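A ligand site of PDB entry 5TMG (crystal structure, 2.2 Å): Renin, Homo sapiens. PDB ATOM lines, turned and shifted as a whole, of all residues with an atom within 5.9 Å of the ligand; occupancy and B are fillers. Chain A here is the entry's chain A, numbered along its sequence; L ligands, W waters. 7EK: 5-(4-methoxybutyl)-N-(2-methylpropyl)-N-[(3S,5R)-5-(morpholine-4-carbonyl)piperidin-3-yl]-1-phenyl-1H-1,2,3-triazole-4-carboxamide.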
ATOM      1  N   THR A  15      -3.158   8.497   3.529  1.00  0.00           N
ATOM      2  CA  THR A  15      -4.490   9.053   3.677  1.00  0.00           C
ATOM      3  C   THR A  15      -4.555  10.577   3.568  1.00  0.00           C
ATOM      4  O   THR A  15      -5.622  11.125   3.289  1.00  0.00           O
ATOM      5  CB  THR A  15      -5.101   8.639   5.036  1.00  0.00           C
ATOM      6  OG1 THR A  15      -4.239   9.045   6.101  1.00  0.00           O
ATOM      7  CG2 THR A  15      -5.275   7.165   5.087  1.00  0.00           C
ATOM      8  N   GLN A  16      -3.438  11.270   3.812  1.00  0.00           N
ATOM      9  CA  GLN A  16      -3.398  12.720   3.696  1.00  0.00           C
ATOM     10  C   GLN A  16      -2.168  13.124   2.925  1.00  0.00           C
ATOM     11  O   GLN A  16      -1.043  12.717   3.265  1.00  0.00           O
ATOM     12  CB  GLN A  16      -3.389  13.383   5.062  1.00  0.00           C
ATOM     13  CG  GLN A  16      -4.507  12.960   5.996  1.00  0.00           C
ATOM     14  CD  GLN A  16      -4.438  13.678   7.322  1.00  0.00           C
ATOM     15  OE1 GLN A  16      -4.135  14.869   7.372  1.00  0.00           O
ATOM     16  NE2 GLN A  16      -4.727  12.972   8.393  1.00  0.00           N
ATOM     17  N   TYR A  17      -2.384  13.921   1.884  1.00  0.00           N
ATOM     18  CA  TYR A  17      -1.311  14.458   1.072  1.00  0.00           C
ATOM     19  C   TYR A  17      -1.448  15.943   1.100  1.00  0.00           C
ATOM     20  O   TYR A  17      -2.508  16.463   0.779  1.00  0.00           O
ATOM     21  CB  TYR A  17      -1.382  13.968  -0.358  1.00  0.00           C
ATOM     22  CG  TYR A  17      -1.093  12.500  -0.519  1.00  0.00           C
ATOM     23  CD1 TYR A  17      -2.073  11.544  -0.274  1.00  0.00           C
ATOM     24  CD2 TYR A  17       0.161  12.065  -0.942  1.00  0.00           C
ATOM     25  CE1 TYR A  17      -1.806  10.202  -0.437  1.00  0.00           C
ATOM     26  CE2 TYR A  17       0.421  10.733  -1.113  1.00  0.00           C
ATOM     27  CZ  TYR A  17      -0.555   9.799  -0.870  1.00  0.00           C
ATOM     28  OH  TYR A  17      -0.281   8.468  -1.052  1.00  0.00           O
ATOM     29  N   TYR A  18      -0.380  16.630   1.486  1.00  0.00           N
ATOM     30  CA  TYR A  18      -0.442  18.056   1.673  1.00  0.00           C
ATOM     31  C   TYR A  18       0.913  18.704   1.414  1.00  0.00           C
ATOM     32  O   TYR A  18       1.939  18.068   1.552  1.00  0.00           O
ATOM     33  CB  TYR A  18      -0.954  18.386   3.084  1.00  0.00           C
ATOM     34  CG  TYR A  18      -0.127  17.809   4.195  1.00  0.00           C
ATOM     35  CD1 TYR A  18       0.998  18.476   4.676  1.00  0.00           C
ATOM     36  CD2 TYR A  18      -0.477  16.603   4.803  1.00  0.00           C
ATOM     37  CE1 TYR A  18       1.757  17.945   5.710  1.00  0.00           C
ATOM     38  CE2 TYR A  18       0.283  16.071   5.837  1.00  0.00           C
ATOM     39  CZ  TYR A  18       1.387  16.748   6.284  1.00  0.00           C
ATOM     40  OH  TYR A  18       2.148  16.211   7.309  1.00  0.00           O
ATOM     41  N   VAL A  33      -4.053  20.757   1.799  1.00  0.00           N
ATOM     42  CA  VAL A  33      -4.446  19.775   0.806  1.00  0.00           C
ATOM     43  C   VAL A  33      -4.791  20.524  -0.455  1.00  0.00           C
ATOM     44  O   VAL A  33      -5.529  21.508  -0.416  1.00  0.00           O
ATOM     45  CB  VAL A  33      -5.684  18.998   1.267  1.00  0.00           C
ATOM     46  CG1 VAL A  33      -6.287  18.171   0.124  1.00  0.00           C
ATOM     47  CG2 VAL A  33      -5.319  18.106   2.444  1.00  0.00           C
ATOM     48  N   ASP A  35      -6.905  20.295  -3.606  1.00  0.00           N
ATOM     49  CA  ASP A  35      -8.171  19.595  -3.759  1.00  0.00           C
ATOM     50  C   ASP A  35      -8.871  19.968  -5.078  1.00  0.00           C
ATOM     51  O   ASP A  35      -9.481  21.028  -5.167  1.00  0.00           O
ATOM     52  CB  ASP A  35      -9.060  19.972  -2.560  1.00  0.00           C
ATOM     53  CG  ASP A  35     -10.460  19.387  -2.654  1.00  0.00           C
ATOM     54  OD1 ASP A  35     -10.671  18.421  -3.412  1.00  0.00           O
ATOM     55  OD2 ASP A  35     -11.356  19.912  -1.945  1.00  0.00           O
ATOM     56  N   THR A  36      -8.812  19.075  -6.073  1.00  0.00           N
ATOM     57  CA  THR A  36      -9.547  19.274  -7.316  1.00  0.00           C
ATOM     58  C   THR A  36     -11.068  19.153  -7.194  1.00  0.00           C
ATOM     59  O   THR A  36     -11.771  19.572  -8.107  1.00  0.00           O
ATOM     60  CB  THR A  36      -9.061  18.324  -8.424  1.00  0.00           C
ATOM     61  OG1 THR A  36      -9.151  16.957  -7.984  1.00  0.00           O
ATOM     62  CG2 THR A  36      -7.627  18.664  -8.805  1.00  0.00           C
ATOM     63  N   GLY A  37     -11.562  18.610  -6.082  1.00  0.00           N
ATOM     64  CA  GLY A  37     -12.995  18.527  -5.837  1.00  0.00           C
ATOM     65  C   GLY A  37     -13.619  19.743  -5.172  1.00  0.00           C
ATOM     66  O   GLY A  37     -14.807  19.718  -4.867  1.00  0.00           O
ATOM     67  N   SER A  38     -12.821  20.781  -4.905  1.00  0.00           N
ATOM     68  CA  SER A  38     -13.373  22.074  -4.474  1.00  0.00           C
ATOM     69  C   SER A  38     -12.567  23.220  -5.068  1.00  0.00           C
ATOM     70  O   SER A  38     -11.530  23.011  -5.688  1.00  0.00           O
ATOM     71  CB  SER A  38     -13.403  22.169  -2.965  1.00  0.00           C
ATOM     72  OG  SER A  38     -12.117  22.105  -2.405  1.00  0.00           O
ATOM     73  N   TRP A  42      -8.815  28.053   1.882  1.00  0.00           N
ATOM     74  CA  TRP A  42      -9.008  28.487   3.248  1.00  0.00           C
ATOM     75  C   TRP A  42      -7.929  27.963   4.180  1.00  0.00           C
ATOM     76  O   TRP A  42      -7.305  26.947   3.916  1.00  0.00           O
ATOM     77  CB  TRP A  42     -10.382  28.081   3.767  1.00  0.00           C
ATOM     78  CG  TRP A  42     -10.599  26.598   3.938  1.00  0.00           C
ATOM     79  CD1 TRP A  42     -11.153  25.748   3.037  1.00  0.00           C
ATOM     80  CD2 TRP A  42     -10.274  25.816   5.096  1.00  0.00           C
ATOM     81  NE1 TRP A  42     -11.194  24.484   3.550  1.00  0.00           N
ATOM     82  CE2 TRP A  42     -10.661  24.490   4.807  1.00  0.00           C
ATOM     83  CE3 TRP A  42      -9.707  26.098   6.343  1.00  0.00           C
ATOM     84  CZ2 TRP A  42     -10.492  23.449   5.725  1.00  0.00           C
ATOM     85  CZ3 TRP A  42      -9.524  25.058   7.250  1.00  0.00           C
ATOM     86  CH2 TRP A  42      -9.932  23.762   6.939  1.00  0.00           C
ATOM     87  N   ARG A  79     -19.208  23.696   2.716  1.00  0.00           N
ATOM     88  CA  ARG A  79     -19.802  22.431   3.107  1.00  0.00           C
ATOM     89  C   ARG A  79     -19.229  21.320   2.254  1.00  0.00           C
ATOM     90  O   ARG A  79     -19.626  21.140   1.099  1.00  0.00           O
ATOM     91  CB  ARG A  79     -21.318  22.485   2.944  1.00  0.00           C
ATOM     92  CG  ARG A  79     -21.981  23.313   4.021  1.00  0.00           C
ATOM     93  CD  ARG A  79     -23.432  23.625   3.718  1.00  0.00           C
ATOM     94  NE  ARG A  79     -24.184  22.416   3.416  1.00  0.00           N
ATOM     95  CZ  ARG A  79     -25.479  22.392   3.120  1.00  0.00           C
ATOM     96  NH1 ARG A  79     -26.190  23.512   3.096  1.00  0.00           N
ATOM     97  NH2 ARG A  79     -26.070  21.223   2.864  1.00  0.00           N
ATOM     98  N   TYR A  80     -18.289  20.584   2.834  1.00  0.00           N
ATOM     99  CA  TYR A  80     -17.761  19.405   2.201  1.00  0.00           C
ATOM    100  C   TYR A  80     -18.608  18.209   2.555  1.00  0.00           C
ATOM    101  O   TYR A  80     -19.430  18.265   3.469  1.00  0.00           O
ATOM    102  CB  TYR A  80     -16.327  19.144   2.637  1.00  0.00           C
ATOM    103  CG  TYR A  80     -15.378  20.262   2.363  1.00  0.00           C
ATOM    104  CD1 TYR A  80     -14.864  20.455   1.089  1.00  0.00           C
ATOM    105  CD2 TYR A  80     -14.957  21.114   3.376  1.00  0.00           C
ATOM    106  CE1 TYR A  80     -13.972  21.469   0.815  1.00  0.00           C
ATOM    107  CE2 TYR A  80     -14.061  22.129   3.127  1.00  0.00           C
ATOM    108  CZ  TYR A  80     -13.576  22.312   1.841  1.00  0.00           C
ATOM    109  OH  TYR A  80     -12.691  23.315   1.587  1.00  0.00           O
ATOM    110  N   SER A  81     -18.391  17.113   1.842  1.00  0.00           N
ATOM    111  CA  SER A  81     -19.121  15.871   2.124  1.00  0.00           C
ATOM    112  C   SER A  81     -18.741  15.262   3.490  1.00  0.00           C
ATOM    113  O   SER A  81     -19.499  14.481   4.029  1.00  0.00           O
ATOM    114  CB  SER A  81     -18.858  14.872   1.002  1.00  0.00           C
ATOM    115  OG  SER A  81     -17.460  14.743   0.809  1.00  0.00           O
ATOM    116  N   THR A  82     -17.581  15.637   4.027  1.00  0.00           N
ATOM    117  CA  THR A  82     -17.064  15.088   5.265  1.00  0.00           C
ATOM    118  C   THR A  82     -17.170  16.046   6.439  1.00  0.00           C
ATOM    119  O   THR A  82     -16.801  15.705   7.563  1.00  0.00           O
ATOM    120  CB  THR A  82     -15.588  14.752   5.090  1.00  0.00           C
ATOM    121  OG1 THR A  82     -14.915  15.900   4.571  1.00  0.00           O
ATOM    122  CG2 THR A  82     -15.419  13.596   4.119  1.00  0.00           C
ATOM    123  N   PRO A 115     -13.955  16.458  10.769  1.00  0.00           N
ATOM    124  CA  PRO A 115     -12.740  15.650  10.724  1.00  0.00           C
ATOM    125  C   PRO A 115     -11.410  16.381  11.097  1.00  0.00           C
ATOM    126  O   PRO A 115     -10.349  15.766  11.032  1.00  0.00           O
ATOM    127  CB  PRO A 115     -12.679  15.280   9.258  1.00  0.00           C
ATOM    128  CG  PRO A 115     -13.184  16.515   8.582  1.00  0.00           C
ATOM    129  CD  PRO A 115     -14.201  17.124   9.483  1.00  0.00           C
ATOM    130  N   PHE A 116     -11.456  17.652  11.452  1.00  0.00           N
ATOM    131  CA  PHE A 116     -10.228  18.445  11.404  1.00  0.00           C
ATOM    132  C   PHE A 116      -9.233  18.216  12.514  1.00  0.00           C
ATOM    133  O   PHE A 116      -8.068  18.455  12.305  1.00  0.00           O
ATOM    134  CB  PHE A 116     -10.531  19.922  11.180  1.00  0.00           C
ATOM    135  CG  PHE A 116     -11.248  20.159   9.889  1.00  0.00           C
ATOM    136  CD1 PHE A 116     -10.565  20.078   8.690  1.00  0.00           C
ATOM    137  CD2 PHE A 116     -12.612  20.427   9.872  1.00  0.00           C
ATOM    138  CE1 PHE A 116     -11.219  20.267   7.490  1.00  0.00           C
ATOM    139  CE2 PHE A 116     -13.267  20.602   8.669  1.00  0.00           C
ATOM    140  CZ  PHE A 116     -12.566  20.524   7.484  1.00  0.00           C
ATOM    141  N   LEU A 118      -8.330  15.333  13.070  1.00  0.00           N
ATOM    142  CA  LEU A 118      -7.604  14.228  12.480  1.00  0.00           C
ATOM    143  C   LEU A 118      -6.699  14.669  11.330  1.00  0.00           C
ATOM    144  O   LEU A 118      -5.942  13.855  10.792  1.00  0.00           O
ATOM    145  CB  LEU A 118      -8.588  13.156  12.025  1.00  0.00           C
ATOM    146  CG  LEU A 118      -9.449  12.589  13.169  1.00  0.00           C
ATOM    147  CD1 LEU A 118     -10.565  11.731  12.622  1.00  0.00           C
ATOM    148  CD2 LEU A 118      -8.589  11.773  14.130  1.00  0.00           C
ATOM    149  N   ALA A 119      -6.745  15.957  10.969  1.00  0.00           N
ATOM    150  CA  ALA A 119      -5.999  16.468   9.833  1.00  0.00           C
ATOM    151  C   ALA A 119      -4.601  16.885  10.282  1.00  0.00           C
ATOM    152  O   ALA A 119      -4.456  17.639  11.256  1.00  0.00           O
ATOM    153  CB  ALA A 119      -6.717  17.651   9.183  1.00  0.00           C
ATOM    154  N   GLU A 120      -3.599  16.398   9.551  1.00  0.00           N
ATOM    155  CA  GLU A 120      -2.233  16.932   9.625  1.00  0.00           C
ATOM    156  C   GLU A 120      -2.122  18.262   8.921  1.00  0.00           C
ATOM    157  O   GLU A 120      -1.261  19.062   9.248  1.00  0.00           O
ATOM    158  CB  GLU A 120      -1.228  15.968   9.008  1.00  0.00           C
ATOM    159  CG  GLU A 120      -0.884  14.813   9.909  1.00  0.00           C
ATOM    160  CD  GLU A 120      -0.168  15.241  11.191  1.00  0.00           C
ATOM    161  OE1 GLU A 120       0.447  16.340  11.230  1.00  0.00           O
ATOM    162  OE2 GLU A 120      -0.232  14.478  12.166  1.00  0.00           O
ATOM    163  N   PHE A 121      -2.985  18.484   7.945  1.00  0.00           N
ATOM    164  CA  PHE A 121      -3.045  19.742   7.214  1.00  0.00           C
ATOM    165  C   PHE A 121      -3.895  20.757   7.991  1.00  0.00           C
ATOM    166  O   PHE A 121      -4.748  20.392   8.818  1.00  0.00           O
ATOM    167  CB  PHE A 121      -3.609  19.540   5.804  1.00  0.00           C
ATOM    168  CG  PHE A 121      -5.013  18.971   5.772  1.00  0.00           C
ATOM    169  CD1 PHE A 121      -5.222  17.585   5.770  1.00  0.00           C
ATOM    170  CD2 PHE A 121      -6.111  19.807   5.744  1.00  0.00           C
ATOM    171  CE1 PHE A 121      -6.489  17.063   5.764  1.00  0.00           C
ATOM    172  CE2 PHE A 121      -7.394  19.276   5.717  1.00  0.00           C
ATOM    173  CZ  PHE A 121      -7.584  17.907   5.731  1.00  0.00           C
ATOM    174  N   VAL A 124      -7.076  24.101   3.018  1.00  0.00           N
ATOM    175  CA  VAL A 124      -7.290  23.541   1.697  1.00  0.00           C
ATOM    176  C   VAL A 124      -7.076  24.593   0.636  1.00  0.00           C
ATOM    177  O   VAL A 124      -7.479  25.755   0.814  1.00  0.00           O
ATOM    178  CB  VAL A 124      -8.729  22.983   1.567  1.00  0.00           C
ATOM    179  CG1 VAL A 124      -8.990  22.406   0.176  1.00  0.00           C
ATOM    180  CG2 VAL A 124      -9.006  21.928   2.631  1.00  0.00           C
ATOM    181  N   GLN A 132     -17.634  26.268  -9.129  1.00  0.00           N
ATOM    182  CA  GLN A 132     -17.877  25.605  -7.849  1.00  0.00           C
ATOM    183  C   GLN A 132     -17.446  26.440  -6.642  1.00  0.00           C
ATOM    184  O   GLN A 132     -17.611  25.984  -5.500  1.00  0.00           O
ATOM    185  CB  GLN A 132     -17.128  24.259  -7.777  1.00  0.00           C
ATOM    186  CG  GLN A 132     -17.852  23.075  -8.419  1.00  0.00           C
ATOM    187  CD  GLN A 132     -17.212  21.735  -8.040  1.00  0.00           C
ATOM    188  OE1 GLN A 132     -16.092  21.672  -7.482  1.00  0.00           O
ATOM    189  NE2 GLN A 132     -17.930  20.649  -8.323  1.00  0.00           N
ATOM    190  N   TYR A 159       1.104  11.298  -6.387  1.00  0.00           N
ATOM    191  CA  TYR A 159       1.027  10.904  -4.982  1.00  0.00           C
ATOM    192  C   TYR A 159       1.813   9.634  -4.809  1.00  0.00           C
ATOM    193  O   TYR A 159       1.507   8.625  -5.430  1.00  0.00           O
ATOM    194  CB  TYR A 159      -0.437  10.651  -4.555  1.00  0.00           C
ATOM    195  CG  TYR A 159      -1.295  11.874  -4.271  1.00  0.00           C
ATOM    196  CD1 TYR A 159      -0.761  13.157  -4.173  1.00  0.00           C
ATOM    197  CD2 TYR A 159      -2.668  11.734  -4.088  1.00  0.00           C
ATOM    198  CE1 TYR A 159      -1.569  14.265  -3.913  1.00  0.00           C
ATOM    199  CE2 TYR A 159      -3.480  12.839  -3.814  1.00  0.00           C
ATOM    200  CZ  TYR A 159      -2.916  14.092  -3.729  1.00  0.00           C
ATOM    201  OH  TYR A 159      -3.683  15.202  -3.464  1.00  0.00           O
ATOM    202  N   LEU A 221     -15.750  11.865 -10.312  1.00  0.00           N
ATOM    203  CA  LEU A 221     -14.995  13.060  -9.951  1.00  0.00           C
ATOM    204  C   LEU A 221     -13.544  12.636  -9.671  1.00  0.00           C
ATOM    205  O   LEU A 221     -13.299  11.673  -8.962  1.00  0.00           O
ATOM    206  CB  LEU A 221     -15.626  13.721  -8.733  1.00  0.00           C
ATOM    207  CG  LEU A 221     -14.928  15.005  -8.258  1.00  0.00           C
ATOM    208  CD1 LEU A 221     -15.285  16.211  -9.122  1.00  0.00           C
ATOM    209  CD2 LEU A 221     -15.315  15.257  -6.812  1.00  0.00           C
ATOM    210  N   ASP A 223     -10.660  13.536  -7.699  1.00  0.00           N
ATOM    211  CA  ASP A 223     -10.627  14.359  -6.497  1.00  0.00           C
ATOM    212  C   ASP A 223      -9.329  14.179  -5.724  1.00  0.00           C
ATOM    213  O   ASP A 223      -9.203  13.277  -4.918  1.00  0.00           O
ATOM    214  CB  ASP A 223     -11.808  14.041  -5.582  1.00  0.00           C
ATOM    215  CG  ASP A 223     -11.901  15.005  -4.410  1.00  0.00           C
ATOM    216  OD1 ASP A 223     -10.986  15.841  -4.233  1.00  0.00           O
ATOM    217  OD2 ASP A 223     -12.913  14.966  -3.668  1.00  0.00           O
ATOM    218  N   THR A 224      -8.394  15.095  -5.937  1.00  0.00           N
ATOM    219  CA  THR A 224      -7.085  14.995  -5.326  1.00  0.00           C
ATOM    220  C   THR A 224      -7.109  15.252  -3.826  1.00  0.00           C
ATOM    221  O   THR A 224      -6.153  14.942  -3.141  1.00  0.00           O
ATOM    222  CB  THR A 224      -6.113  16.009  -5.950  1.00  0.00           C
ATOM    223  OG1 THR A 224      -6.643  17.331  -5.754  1.00  0.00           O
ATOM    224  CG2 THR A 224      -5.890  15.689  -7.450  1.00  0.00           C
ATOM    225  N   GLY A 225      -8.198  15.860  -3.336  1.00  0.00           N
ATOM    226  CA  GLY A 225      -8.360  16.151  -1.929  1.00  0.00           C
ATOM    227  C   GLY A 225      -9.078  15.084  -1.145  1.00  0.00           C
ATOM    228  O   GLY A 225      -9.375  15.299   0.012  1.00  0.00           O
ATOM    229  N   ALA A 226      -9.370  13.944  -1.773  1.00  0.00           N
ATOM    230  CA  ALA A 226     -10.007  12.802  -1.107  1.00  0.00           C
ATOM    231  C   ALA A 226      -8.998  11.679  -0.901  1.00  0.00           C
ATOM    232  O   ALA A 226      -8.116  11.473  -1.730  1.00  0.00           O
ATOM    233  CB  ALA A 226     -11.169  12.314  -1.945  1.00  0.00           C
ATOM    234  N   SER A 227      -9.132  10.964   0.213  1.00  0.00           N
ATOM    235  CA  SER A 227      -8.216   9.883   0.559  1.00  0.00           C
ATOM    236  C   SER A 227      -8.452   8.637  -0.270  1.00  0.00           C
ATOM    237  O   SER A 227      -7.517   7.947  -0.656  1.00  0.00           O
ATOM    238  CB  SER A 227      -8.343   9.505   2.043  1.00  0.00           C
ATOM    239  OG  SER A 227      -8.017  10.608   2.884  1.00  0.00           O
ATOM    240  N   MET A 300     -19.345   7.790  -0.251  1.00  0.00           N
ATOM    241  CA  MET A 300     -19.559   9.234  -0.112  1.00  0.00           C
ATOM    242  C   MET A 300     -20.765   9.581  -0.982  1.00  0.00           C
ATOM    243  O   MET A 300     -20.691   9.503  -2.205  1.00  0.00           O
ATOM    244  CB  MET A 300     -18.326  10.053  -0.528  1.00  0.00           C
ATOM    245  CG  MET A 300     -17.469  10.577   0.626  1.00  0.00           C
ATOM    246  SD  MET A 300     -15.997  11.504   0.113  1.00  0.00           S
ATOM    247  CE  MET A 300     -16.665  12.597  -1.149  1.00  0.00           C
ATOM    248  N   ILE A 302     -22.828  12.188  -2.542  1.00  0.00           N
ATOM    249  CA  ILE A 302     -22.650  13.575  -2.946  1.00  0.00           C
ATOM    250  C   ILE A 302     -23.952  14.003  -3.595  1.00  0.00           C
ATOM    251  O   ILE A 302     -24.437  13.323  -4.501  1.00  0.00           O
ATOM    252  CB  ILE A 302     -21.444  13.716  -3.897  1.00  0.00           C
ATOM    253  CG1 ILE A 302     -20.150  13.344  -3.142  1.00  0.00           C
ATOM    254  CG2 ILE A 302     -21.348  15.131  -4.453  1.00  0.00           C
ATOM    255  CD1 ILE A 302     -18.988  13.006  -4.044  1.00  0.00           C
ATOM    256  N   PRO A 303     -24.550  15.124  -3.129  1.00  0.00           N
ATOM    257  CA  PRO A 303     -25.853  15.502  -3.683  1.00  0.00           C
ATOM    258  C   PRO A 303     -25.722  16.167  -5.055  1.00  0.00           C
ATOM    259  O   PRO A 303     -24.622  16.570  -5.444  1.00  0.00           O
ATOM    260  CB  PRO A 303     -26.395  16.491  -2.658  1.00  0.00           C
ATOM    261  CG  PRO A 303     -25.224  16.980  -1.892  1.00  0.00           C
ATOM    262  CD  PRO A 303     -24.028  16.147  -2.203  1.00  0.00           C
ATOM    263  N   THR A 306     -23.605  17.907  -8.525  1.00  0.00           N
ATOM    264  CA  THR A 306     -22.325  17.205  -8.679  1.00  0.00           C
ATOM    265  C   THR A 306     -22.494  15.694  -8.628  1.00  0.00           C
ATOM    266  O   THR A 306     -21.861  14.967  -9.402  1.00  0.00           O
ATOM    267  CB  THR A 306     -21.306  17.630  -7.603  1.00  0.00           C
ATOM    268  OG1 THR A 306     -21.155  19.045  -7.642  1.00  0.00           O
ATOM    269  CG2 THR A 306     -19.950  16.972  -7.825  1.00  0.00           C
ATOM    270  N   THR A 309     -22.165  10.509  -7.517  1.00  0.00           N
ATOM    271  CA  THR A 309     -20.962  10.327  -8.323  1.00  0.00           C
ATOM    272  C   THR A 309     -19.933   9.475  -7.592  1.00  0.00           C
ATOM    273  O   THR A 309     -19.852   9.485  -6.360  1.00  0.00           O
ATOM    274  CB  THR A 309     -20.333  11.696  -8.706  1.00  0.00           C
ATOM    275  OG1 THR A 309     -19.164  11.502  -9.510  1.00  0.00           O
ATOM    276  CG2 THR A 309     -19.951  12.524  -7.477  1.00  0.00           C
ATOM    277  N   ALA A 314      -6.943   9.590  -3.623  1.00  0.00           N
ATOM    278  CA  ALA A 314      -5.533   9.193  -3.536  1.00  0.00           C
ATOM    279  C   ALA A 314      -5.291   7.726  -3.875  1.00  0.00           C
ATOM    280  O   ALA A 314      -4.300   7.400  -4.509  1.00  0.00           O
ATOM    281  CB  ALA A 314      -4.960   9.512  -2.168  1.00  0.00           C
HETATM  282  C4  7EK L   1      -6.741  14.255   2.787  1.00  0.00           C
HETATM  283  C5  7EK L   1      -8.084  14.865   3.213  1.00  0.00           C
HETATM  284  C6  7EK L   1      -9.224  13.839   3.067  1.00  0.00           C
HETATM  285  C7  7EK L   1     -10.392  14.309   3.905  1.00  0.00           C
HETATM  286  C8  7EK L   1     -11.582  14.830   3.442  1.00  0.00           C
HETATM  287  C13 7EK L   1      -8.990  12.657   6.202  1.00  0.00           C
HETATM  288  C15 7EK L   1      -7.903  13.081   8.310  1.00  0.00           C
HETATM  289  C17 7EK L   1      -9.360  14.755   7.372  1.00  0.00           C
HETATM  290  C21 7EK L   1     -12.448  17.504   2.255  1.00  0.00           C
HETATM  291  C22 7EK L   1     -11.108  17.954   2.867  1.00  0.00           C
HETATM  292  C24 7EK L   1     -11.383  19.147   3.784  1.00  0.00           C
HETATM  293  C1  7EK L   1      -5.275  13.543  -0.524  1.00  0.00           C
HETATM  294  O2  7EK L   1      -5.264  13.991   0.828  1.00  0.00           O
HETATM  295  C3  7EK L   1      -6.551  14.392   1.280  1.00  0.00           C
HETATM  296  N9  7EK L   1     -12.351  15.127   4.494  1.00  0.00           N
HETATM  297  N10 7EK L   1     -11.742  14.854   5.574  1.00  0.00           N
HETATM  298  N11 7EK L   1     -10.489  14.334   5.268  1.00  0.00           N
HETATM  299  C12 7EK L   1      -9.598  13.922   6.267  1.00  0.00           C
HETATM  300  C14 7EK L   1      -8.138  12.236   7.225  1.00  0.00           C
HETATM  301  C16 7EK L   1      -8.504  14.336   8.382  1.00  0.00           C
HETATM  302  C18 7EK L   1     -12.047  15.032   2.044  1.00  0.00           C
HETATM  303  O19 7EK L   1     -12.116  14.030   1.358  1.00  0.00           O
HETATM  304  N20 7EK L   1     -12.448  16.219   1.501  1.00  0.00           N
HETATM  305  C23 7EK L   1     -10.051  18.328   1.822  1.00  0.00           C
HETATM  306  C25 7EK L   1     -12.934  16.186   0.088  1.00  0.00           C
HETATM  307  C27 7EK L   1     -12.074  17.066  -0.829  1.00  0.00           C
HETATM  308  N28 7EK L   1     -12.688  17.198  -2.179  1.00  0.00           N
HETATM  309  C29 7EK L   1     -14.049  17.779  -2.101  1.00  0.00           C
HETATM  310  C30 7EK L   1     -14.959  16.776  -1.389  1.00  0.00           C
HETATM  311  C31 7EK L   1     -14.437  16.551   0.058  1.00  0.00           C
HETATM  312  C32 7EK L   1     -16.389  17.277  -1.378  1.00  0.00           C
HETATM  313  O33 7EK L   1     -16.737  17.960  -0.434  1.00  0.00           O
HETATM  314  N34 7EK L   1     -17.294  16.995  -2.363  1.00  0.00           N
HETATM  315  C35 7EK L   1     -16.974  16.176  -3.560  1.00  0.00           C
HETATM  316  C36 7EK L   1     -17.275  17.104  -4.763  1.00  0.00           C
HETATM  317  O37 7EK L   1     -18.650  17.514  -4.695  1.00  0.00           O
HETATM  318  C38 7EK L   1     -19.012  18.314  -3.551  1.00  0.00           C
HETATM  319  C39 7EK L   1     -18.688  17.520  -2.276  1.00  0.00           C
HETATM  320  O   HOH W   1     -11.352  11.469   1.834  1.00  0.00           O
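OG1 of Thr 82 is in hydrogen-bond range of N9 of the ligand (2.7 Å). The side-chain carboxylate of Asp 35 lies within salt-bridge range of a nitrogen (N28) of the ligand (2.7 Å). A nitrogen (N28) of the ligand is in salt-bridge range of the side-chain carboxylate of Asp 223, 2.7 Å away. The backbone NH (N) of Tyr 17 lies within hydrogen-bond range of an oxygen (O2) of the ligand (3.1 Å). The backbone NH (N) of Ser 81 is in hydrogen-bond range of an oxygen (O33) of the ligand.
The backbone carbonyl oxygen (O) of Val 124 lies within hydrogen-bond range of the backbone NH (N) of Trp 42, at 2.9 Å. The backbone NH (N) of Gly 37 lies within hydrogen-bond range of the side-chain carboxylate (OD1) of Asp 223, 3.4 Å away. The side-chain carboxylate of Asp 35 lies close to the backbone NH of Ser 38, at 3.4 Å. The side-chain amide nitrogen (NE2) of Gln 16 sits at hydrogen-bond distance from the backbone carbonyl oxygen (O) of Leu 118 (2.8 Å). O of Thr 224 sits at hydrogen-bond distance from OH of Tyr 159. The backbone NH of Glu 120 is in hydrogen-bond range of the side-chain amide oxygen of Gln 16 (2.7 Å). O of Ser 227 sits close to N of Ala 314 (3.4 Å). SD of Met 300 lies close to OG of Ser 81 (3.6 Å).
An oxygen (O19) of the ligand lies close to the backbone carbonyl oxygen of Gly 225 (3.3 Å). Residues that only touch the ligand: Thr 15 (3.4 Å), Gln 16 (3.2 Å), Val 33 (3.96 Å), Gly 37 (3.5 Å), Tyr 80 (3.2 Å), Pro 115 (3.5 Å), Phe 116 (3.9 Å), Leu 118 (3.3 Å), Ala 119 (3.5 Å), Phe 121 (3.7 Å), Val 124 (3.8 Å), Tyr 159 (3.7 Å), Leu 221 (3.4 Å), Thr 224 (3.1 Å), Ala 226 (3.5 Å), Ser 227 (3.5 Å), Ile 302 (3.6 Å) and Thr 306 (3.4 Å). Hydrophobic or aromatic side chains that line the ligand: Tyr 17, Val 33, Tyr 80, Pro 115, Phe 116, Leu 118, Ala 119, Phe 121, Val 124, Tyr 159, Leu 221, Ala 226 and Ile 302. Of the 35 residues printed, 24 come within 4 Å of the ligand.
Water W1 lies within hydrogen-bond range of O19 of the ligand (2.7 Å) and N of Ser 227 (2.8 Å).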
